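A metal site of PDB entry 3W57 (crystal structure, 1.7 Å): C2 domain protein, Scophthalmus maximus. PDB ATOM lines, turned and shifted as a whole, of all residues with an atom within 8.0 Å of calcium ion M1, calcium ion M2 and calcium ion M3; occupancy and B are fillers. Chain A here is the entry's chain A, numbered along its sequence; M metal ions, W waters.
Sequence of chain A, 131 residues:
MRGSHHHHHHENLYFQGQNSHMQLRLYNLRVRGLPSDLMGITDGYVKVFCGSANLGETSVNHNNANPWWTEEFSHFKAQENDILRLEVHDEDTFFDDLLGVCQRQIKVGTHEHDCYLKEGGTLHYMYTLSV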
ATOM      1  N   SER A  36     -17.670 -15.204  26.411  1.00  0.00           N
ATOM      2  CA  SER A  36     -16.332 -15.066  25.856  1.00  0.00           C
ATOM      3  C   SER A  36     -15.514 -16.341  26.087  1.00  0.00           C
ATOM      4  O   SER A  36     -15.698 -17.045  27.074  1.00  0.00           O
ATOM      5  CB  SER A  36     -15.618 -13.887  26.542  1.00  0.00           C
ATOM      6  OG  SER A  36     -14.322 -13.636  26.000  1.00  0.00           O
ATOM      7  N   ASP A  37     -14.617 -16.629  25.155  1.00  0.00           N
ATOM      8  CA  ASP A  37     -13.573 -17.631  25.322  1.00  0.00           C
ATOM      9  C   ASP A  37     -12.456 -16.973  26.157  1.00  0.00           C
ATOM     10  O   ASP A  37     -12.509 -15.785  26.473  1.00  0.00           O
ATOM     11  CB  ASP A  37     -13.043 -18.011  23.924  1.00  0.00           C
ATOM     12  CG  ASP A  37     -12.393 -19.374  23.878  1.00  0.00           C
ATOM     13  OD1 ASP A  37     -12.197 -19.980  24.941  1.00  0.00           O
ATOM     14  OD2 ASP A  37     -12.063 -19.815  22.759  1.00  0.00           O
ATOM     15  N   LEU A  38     -11.454 -17.759  26.522  1.00  0.00           N
ATOM     16  CA  LEU A  38     -10.267 -17.214  27.179  1.00  0.00           C
ATOM     17  C   LEU A  38      -9.632 -16.146  26.287  1.00  0.00           C
ATOM     18  O   LEU A  38      -9.165 -15.110  26.754  1.00  0.00           O
ATOM     19  CB  LEU A  38      -9.282 -18.349  27.439  1.00  0.00           C
ATOM     20  CG  LEU A  38      -7.866 -18.004  27.925  1.00  0.00           C
ATOM     21  CD1 LEU A  38      -7.891 -17.045  29.104  1.00  0.00           C
ATOM     22  CD2 LEU A  38      -7.140 -19.299  28.287  1.00  0.00           C
ATOM     23  N   MET A  39      -9.622 -16.407  24.985  1.00  0.00           N
ATOM     24  CA  MET A  39      -9.136 -15.431  24.025  1.00  0.00           C
ATOM     25  C   MET A  39     -10.120 -15.266  22.889  1.00  0.00           C
ATOM     26  O   MET A  39     -10.067 -16.008  21.908  1.00  0.00           O
ATOM     27  CB  MET A  39      -7.789 -15.879  23.466  1.00  0.00           C
ATOM     28  CG  MET A  39      -6.723 -15.944  24.522  1.00  0.00           C
ATOM     29  SD  MET A  39      -5.157 -16.444  23.815  1.00  0.00           S
ATOM     30  CE  MET A  39      -5.500 -18.155  23.416  1.00  0.00           C
ATOM     31  N   GLY A  40     -11.013 -14.299  23.033  1.00  0.00           N
ATOM     32  CA  GLY A  40     -11.869 -13.912  21.937  1.00  0.00           C
ATOM     33  C   GLY A  40     -13.175 -14.676  21.891  1.00  0.00           C
ATOM     34  O   GLY A  40     -13.661 -15.159  22.904  1.00  0.00           O
ATOM     35  N   ILE A  41     -13.726 -14.807  20.687  1.00  0.00           N
ATOM     36  CA  ILE A  41     -15.077 -15.325  20.533  1.00  0.00           C
ATOM     37  C   ILE A  41     -15.085 -16.845  20.508  1.00  0.00           C
ATOM     38  O   ILE A  41     -14.230 -17.462  19.891  1.00  0.00           O
ATOM     39  CB  ILE A  41     -15.734 -14.742  19.268  1.00  0.00           C
ATOM     40  CG1 ILE A  41     -15.665 -13.212  19.336  1.00  0.00           C
ATOM     41  CG2 ILE A  41     -17.166 -15.231  19.103  1.00  0.00           C
ATOM     42  CD1 ILE A  41     -16.162 -12.505  18.089  1.00  0.00           C
ATOM     43  N   THR A  42     -16.037 -17.432  21.205  1.00  0.00           N
ATOM     44  CA  THR A  42     -16.156 -18.880  21.352  1.00  0.00           C
ATOM     45  C   THR A  42     -16.351 -19.638  20.024  1.00  0.00           C
ATOM     46  O   THR A  42     -16.897 -19.104  19.043  1.00  0.00           O
ATOM     47  CB  THR A  42     -17.284 -19.196  22.345  1.00  0.00           C
ATOM     48  OG1 THR A  42     -16.892 -18.744  23.638  1.00  0.00           O
ATOM     49  CG2 THR A  42     -17.600 -20.671  22.423  1.00  0.00           C
ATOM     50  N   ASP A  43     -15.890 -20.889  20.016  1.00  0.00           N
ATOM     51  CA  ASP A  43     -15.856 -21.739  18.826  1.00  0.00           C
ATOM     52  C   ASP A  43     -16.681 -22.986  19.105  1.00  0.00           C
ATOM     53  O   ASP A  43     -16.151 -24.074  19.377  1.00  0.00           O
ATOM     54  CB  ASP A  43     -14.397 -22.078  18.553  1.00  0.00           C
ATOM     55  CG  ASP A  43     -13.526 -20.847  18.647  1.00  0.00           C
ATOM     56  OD1 ASP A  43     -13.663 -19.997  17.747  1.00  0.00           O
ATOM     57  OD2 ASP A  43     -12.766 -20.695  19.630  1.00  0.00           O
ATOM     58  N   GLY A  44     -17.998 -22.825  19.061  1.00  0.00           N
ATOM     59  CA  GLY A  44     -18.902 -23.851  19.546  1.00  0.00           C
ATOM     60  C   GLY A  44     -19.142 -25.031  18.632  1.00  0.00           C
ATOM     61  O   GLY A  44     -19.128 -24.903  17.403  1.00  0.00           O
ATOM     62  N   VAL A  60     -17.407 -27.293  13.967  1.00  0.00           N
ATOM     63  CA  VAL A  60     -17.152 -26.152  14.836  1.00  0.00           C
ATOM     64  C   VAL A  60     -17.564 -24.889  14.091  1.00  0.00           C
ATOM     65  O   VAL A  60     -17.237 -24.708  12.896  1.00  0.00           O
ATOM     66  CB  VAL A  60     -15.648 -26.084  15.210  1.00  0.00           C
ATOM     67  CG1 VAL A  60     -15.350 -24.842  16.023  1.00  0.00           C
ATOM     68  CG2 VAL A  60     -15.222 -27.330  15.980  1.00  0.00           C
ATOM     69  N   ASN A  61     -18.322 -24.038  14.777  1.00  0.00           N
ATOM     70  CA  ASN A  61     -18.747 -22.770  14.208  1.00  0.00           C
ATOM     71  C   ASN A  61     -17.822 -21.710  14.784  1.00  0.00           C
ATOM     72  O   ASN A  61     -18.052 -21.170  15.863  1.00  0.00           O
ATOM     73  CB  ASN A  61     -20.227 -22.512  14.559  1.00  0.00           C
ATOM     74  CG  ASN A  61     -20.862 -21.487  13.645  1.00  0.00           C
ATOM     75  OD1 ASN A  61     -20.248 -20.497  13.316  1.00  0.00           O
ATOM     76  ND2 ASN A  61     -22.109 -21.741  13.241  1.00  0.00           N
ATOM     77  N   HIS A  62     -16.716 -21.457  14.086  1.00  0.00           N
ATOM     78  CA  HIS A  62     -15.624 -20.663  14.633  1.00  0.00           C
ATOM     79  C   HIS A  62     -15.975 -19.207  14.874  1.00  0.00           C
ATOM     80  O   HIS A  62     -16.674 -18.594  14.060  1.00  0.00           O
ATOM     81  CB  HIS A  62     -14.407 -20.724  13.713  1.00  0.00           C
ATOM     82  CG  HIS A  62     -13.796 -22.089  13.631  1.00  0.00           C
ATOM     83  ND1 HIS A  62     -12.904 -22.549  14.579  1.00  0.00           N
ATOM     84  CD2 HIS A  62     -13.983 -23.112  12.758  1.00  0.00           C
ATOM     85  CE1 HIS A  62     -12.542 -23.788  14.267  1.00  0.00           C
ATOM     86  NE2 HIS A  62     -13.181 -24.140  13.175  1.00  0.00           N
ATOM     87  N   ASN A  63     -15.514 -18.708  16.015  1.00  0.00           N
ATOM     88  CA  ASN A  63     -15.612 -17.280  16.330  1.00  0.00           C
ATOM     89  C   ASN A  63     -17.022 -16.744  16.139  1.00  0.00           C
ATOM     90  O   ASN A  63     -17.226 -15.744  15.439  1.00  0.00           O
ATOM     91  CB  ASN A  63     -14.629 -16.513  15.476  1.00  0.00           C
ATOM     92  CG  ASN A  63     -13.225 -16.939  15.734  1.00  0.00           C
ATOM     93  OD1 ASN A  63     -12.824 -17.045  16.884  1.00  0.00           O
ATOM     94  ND2 ASN A  63     -12.464 -17.237  14.669  1.00  0.00           N
ATOM     95  N   ASN A  64     -17.966 -17.417  16.777  1.00  0.00           N
ATOM     96  CA  ASN A  64     -19.368 -17.079  16.641  1.00  0.00           C
ATOM     97  C   ASN A  64     -20.070 -17.178  17.999  1.00  0.00           C
ATOM     98  O   ASN A  64     -20.185 -18.260  18.558  1.00  0.00           O
ATOM     99  CB  ASN A  64     -20.015 -18.023  15.614  1.00  0.00           C
ATOM    100  CG  ASN A  64     -21.382 -17.538  15.118  1.00  0.00           C
ATOM    101  OD1 ASN A  64     -22.031 -16.717  15.764  1.00  0.00           O
ATOM    102  ND2 ASN A  64     -21.828 -18.086  13.978  1.00  0.00           N
ATOM    103  N   HIS A  89     -19.871 -27.565  23.467  1.00  0.00           N
ATOM    104  CA  HIS A  89     -18.459 -27.421  23.806  1.00  0.00           C
ATOM    105  C   HIS A  89     -17.855 -26.266  23.036  1.00  0.00           C
ATOM    106  O   HIS A  89     -18.316 -25.925  21.954  1.00  0.00           O
ATOM    107  CB  HIS A  89     -17.656 -28.667  23.411  1.00  0.00           C
ATOM    108  CG  HIS A  89     -18.060 -29.926  24.124  1.00  0.00           C
ATOM    109  ND1 HIS A  89     -17.260 -30.523  25.080  1.00  0.00           N
ATOM    110  CD2 HIS A  89     -19.144 -30.723  23.989  1.00  0.00           C
ATOM    111  CE1 HIS A  89     -17.845 -31.623  25.510  1.00  0.00           C
ATOM    112  NE2 HIS A  89     -18.992 -31.776  24.872  1.00  0.00           N
ATOM    113  N   ASP A  90     -16.790 -25.695  23.608  1.00  0.00           N
ATOM    114  CA  ASP A  90     -15.909 -24.778  22.877  1.00  0.00           C
ATOM    115  C   ASP A  90     -14.671 -25.549  22.423  1.00  0.00           C
ATOM    116  O   ASP A  90     -13.986 -26.141  23.259  1.00  0.00           O
ATOM    117  CB  ASP A  90     -15.471 -23.640  23.774  1.00  0.00           C
ATOM    118  CG  ASP A  90     -14.346 -22.823  23.174  1.00  0.00           C
ATOM    119  OD1 ASP A  90     -14.499 -22.332  22.037  1.00  0.00           O
ATOM    120  OD2 ASP A  90     -13.268 -22.713  23.796  1.00  0.00           O
ATOM    121  N   GLU A  91     -14.367 -25.521  21.121  1.00  0.00           N
ATOM    122  CA  GLU A  91     -13.123 -26.113  20.652  1.00  0.00           C
ATOM    123  C   GLU A  91     -11.933 -25.238  21.019  1.00  0.00           C
ATOM    124  O   GLU A  91     -11.953 -24.031  20.782  1.00  0.00           O
ATOM    125  CB  GLU A  91     -13.151 -26.322  19.127  1.00  0.00           C
ATOM    126  CG  GLU A  91     -11.943 -27.097  18.625  1.00  0.00           C
ATOM    127  CD  GLU A  91     -11.793 -27.063  17.112  1.00  0.00           C
ATOM    128  OE1 GLU A  91     -11.840 -28.146  16.494  1.00  0.00           O
ATOM    129  OE2 GLU A  91     -11.617 -25.961  16.550  1.00  0.00           O
ATOM    130  N   ASP A  92     -10.913 -25.858  21.610  1.00  0.00           N
ATOM    131  CA  ASP A  92      -9.649 -25.186  21.896  1.00  0.00           C
ATOM    132  C   ASP A  92      -8.482 -26.067  21.479  1.00  0.00           C
ATOM    133  O   ASP A  92      -8.647 -27.256  21.188  1.00  0.00           O
ATOM    134  CB  ASP A  92      -9.528 -24.911  23.381  1.00  0.00           C
ATOM    135  CG  ASP A  92     -10.181 -23.604  23.804  1.00  0.00           C
ATOM    136  OD1 ASP A  92     -10.163 -22.617  23.039  1.00  0.00           O
ATOM    137  OD2 ASP A  92     -10.661 -23.596  24.937  1.00  0.00           O
ATOM    138  N   THR A  93      -7.296 -25.471  21.429  1.00  0.00           N
ATOM    139  CA  THR A  93      -6.100 -26.195  20.963  1.00  0.00           C
ATOM    140  C   THR A  93      -5.716 -27.394  21.836  1.00  0.00           C
ATOM    141  O   THR A  93      -5.390 -28.471  21.303  1.00  0.00           O
ATOM    142  CB  THR A  93      -4.922 -25.240  20.805  1.00  0.00           C
ATOM    143  OG1 THR A  93      -5.243 -24.274  19.786  1.00  0.00           O
ATOM    144  CG2 THR A  93      -3.678 -26.005  20.372  1.00  0.00           C
ATOM    145  N   PHE A  95      -7.362 -28.384  25.263  1.00  0.00           N
ATOM    146  CA  PHE A  95      -8.494 -29.045  25.929  1.00  0.00           C
ATOM    147  C   PHE A  95      -9.769 -28.310  25.566  1.00  0.00           C
ATOM    148  O   PHE A  95      -9.870 -27.120  25.803  1.00  0.00           O
ATOM    149  CB  PHE A  95      -8.370 -29.014  27.455  1.00  0.00           C
ATOM    150  CG  PHE A  95      -7.090 -29.630  27.980  1.00  0.00           C
ATOM    151  CD1 PHE A  95      -7.026 -30.974  28.288  1.00  0.00           C
ATOM    152  CD2 PHE A  95      -5.969 -28.842  28.160  1.00  0.00           C
ATOM    153  CE1 PHE A  95      -5.841 -31.530  28.777  1.00  0.00           C
ATOM    154  CE2 PHE A  95      -4.782 -29.381  28.648  1.00  0.00           C
ATOM    155  CZ  PHE A  95      -4.723 -30.713  28.960  1.00  0.00           C
ATOM    156  N   ASP A  96     -10.762 -29.020  25.016  1.00  0.00           N
ATOM    157  CA  ASP A  96     -12.055 -28.377  24.751  1.00  0.00           C
ATOM    158  C   ASP A  96     -12.792 -28.151  26.067  1.00  0.00           C
ATOM    159  O   ASP A  96     -12.653 -28.954  27.006  1.00  0.00           O
ATOM    160  CB  ASP A  96     -12.918 -29.242  23.827  1.00  0.00           C
ATOM    161  CG  ASP A  96     -12.384 -29.342  22.423  1.00  0.00           C
ATOM    162  OD1 ASP A  96     -11.378 -28.674  22.096  1.00  0.00           O
ATOM    163  OD2 ASP A  96     -12.970 -30.091  21.611  1.00  0.00           O
ATOM    164  N   ASP A  97     -13.575 -27.076  26.151  1.00  0.00           N
ATOM    165  CA  ASP A  97     -14.313 -26.744  27.368  1.00  0.00           C
ATOM    166  C   ASP A  97     -15.797 -27.056  27.190  1.00  0.00           C
ATOM    167  O   ASP A  97     -16.414 -26.598  26.230  1.00  0.00           O
ATOM    168  CB  ASP A  97     -14.181 -25.262  27.694  1.00  0.00           C
ATOM    169  CG  ASP A  97     -12.791 -24.894  28.122  1.00  0.00           C
ATOM    170  OD1 ASP A  97     -12.276 -25.537  29.062  1.00  0.00           O
ATOM    171  OD2 ASP A  97     -12.197 -23.993  27.491  1.00  0.00           O
ATOM    172  N   LEU A  98     -16.355 -27.794  28.138  1.00  0.00           N
ATOM    173  CA  LEU A  98     -17.780 -28.091  28.088  1.00  0.00           C
ATOM    174  C   LEU A  98     -18.539 -26.939  28.725  1.00  0.00           C
ATOM    175  O   LEU A  98     -18.331 -26.617  29.903  1.00  0.00           O
ATOM    176  CB  LEU A  98     -18.058 -29.440  28.783  1.00  0.00           C
ATOM    177  CG  LEU A  98     -19.508 -29.923  28.896  1.00  0.00           C
ATOM    178  CD1 LEU A  98     -20.288 -29.780  27.586  1.00  0.00           C
ATOM    179  CD2 LEU A  98     -19.517 -31.354  29.351  1.00  0.00           C
ATOM    180  N   LEU A  99     -19.399 -26.283  27.927  1.00  0.00           N
ATOM    181  CA  LEU A  99     -20.093 -25.086  28.374  1.00  0.00           C
ATOM    182  C   LEU A  99     -21.451 -25.364  28.989  1.00  0.00           C
ATOM    183  O   LEU A  99     -21.911 -24.602  29.838  1.00  0.00           O
ATOM    184  CB  LEU A  99     -20.252 -24.098  27.223  1.00  0.00           C
ATOM    185  CG  LEU A  99     -18.992 -23.756  26.429  1.00  0.00           C
ATOM    186  CD1 LEU A  99     -19.328 -22.738  25.355  1.00  0.00           C
ATOM    187  CD2 LEU A  99     -17.892 -23.221  27.324  1.00  0.00           C
HETATM  188 CA    CA M   1     -12.270 -18.286  18.816  1.00  0.00          CA
HETATM  189 CA    CA M   2     -12.040 -21.856  21.666  1.00  0.00          CA
HETATM  190 CA    CA M   3     -12.186 -22.153  26.017  1.00  0.00          CA
HETATM  191  O   HOH W   1     -10.397 -19.559  17.857  1.00  0.00           O
HETATM  192  O   HOH W   2      -9.840 -21.693  27.042  1.00  0.00           O
HETATM  193  O   HOH W   3     -14.589 -22.043  26.688  1.00  0.00           O
HETATM  194  O   HOH W   4      -9.943 -21.272  20.296  1.00  0.00           O
HETATM  195  O   HOH W   5     -11.141 -18.099  20.965  1.00  0.00           O
HETATM  196  O   HOH W   6     -10.692 -16.394  18.613  1.00  0.00           O
HETATM  197  O   HOH W   7     -12.355 -20.594  27.983  1.00  0.00           O
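Calcium ion M2 is bound by the side-chain carboxylate (OD2) of Asp 37 (2.3 Å), the backbone carbonyl oxygen (O) of Glu 91 (2.3 Å), the side-chain carboxylate (OD1) of Asp 92 (2.4 Å), the side-chain carboxylate (OD2) of Asp 43 (2.5 Å), the side-chain carboxylate (OD1) of Asp 90 (2.5 Å), water W4 (2.6 Å) and the side-chain carboxylate (OD2) of Asp 90 (2.6 Å).
Calcium ion M2 has seven donor atoms within binding distance.
Calcium ion M3 is bound by the side-chain carboxylate (OD2) of Asp 97 (2.4 Å), the side-chain carboxylate (OD2) of Asp 92 (2.4 Å), the side-chain carboxylate (OD1) of Asp 37 (2.4 Å), water W3 (2.5 Å), water W7 (2.5 Å), the side-chain carboxylate (OD2) of Asp 90 (2.5 Å) and water W2 (2.6 Å).
Of the 24 residues printed, 5 come within 4 Å of calcium ion M2.
Along chain A the residues within 4 Å of calcium ion M2 span positions 37 to 92.
The nearest printed residue that does not touch calcium ion M2 is Thr 42 (5.1 Å).
Within 4 Å of calcium ion M1: Ile 41, Asp 43 and Asn 63.
OG1 of Thr 42 sits at hydrogen-bond distance from N of Asp 37 (3.5 Å).
The backbone NH of Asp 92 is in hydrogen-bond range of the side-chain carboxylate of Asp 96, 2.9 Å away.
The backbone NH of Asn 63 lies within hydrogen-bond range of the backbone carbonyl oxygen of Thr 42, 3.4 Å away.
Four residues have an atom within 4 Å of calcium ion M3: Asp 37, Asp 90, Asp 92 and Asp 97.
The nearest printed residue that does not touch calcium ion M3 is Leu 38 (4.5 Å).
Calcium ion M1 is bound by OD1 of Asn 63.
O of Ile 41 binds calcium ion M1.
Water W5 binds calcium ion M1, 2.4 Å away.
OD1 of Asp 43 binds calcium ion M1.
Water W1 is bound to calcium ion M1, at 2.5 Å.
Calcium ion M1 is bound by water W6.
Calcium ion M1 is bound by the side-chain carboxylate (OD2) of Asp 43 (2.6 Å).
Calcium ion M1 has seven donor atoms within binding distance.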
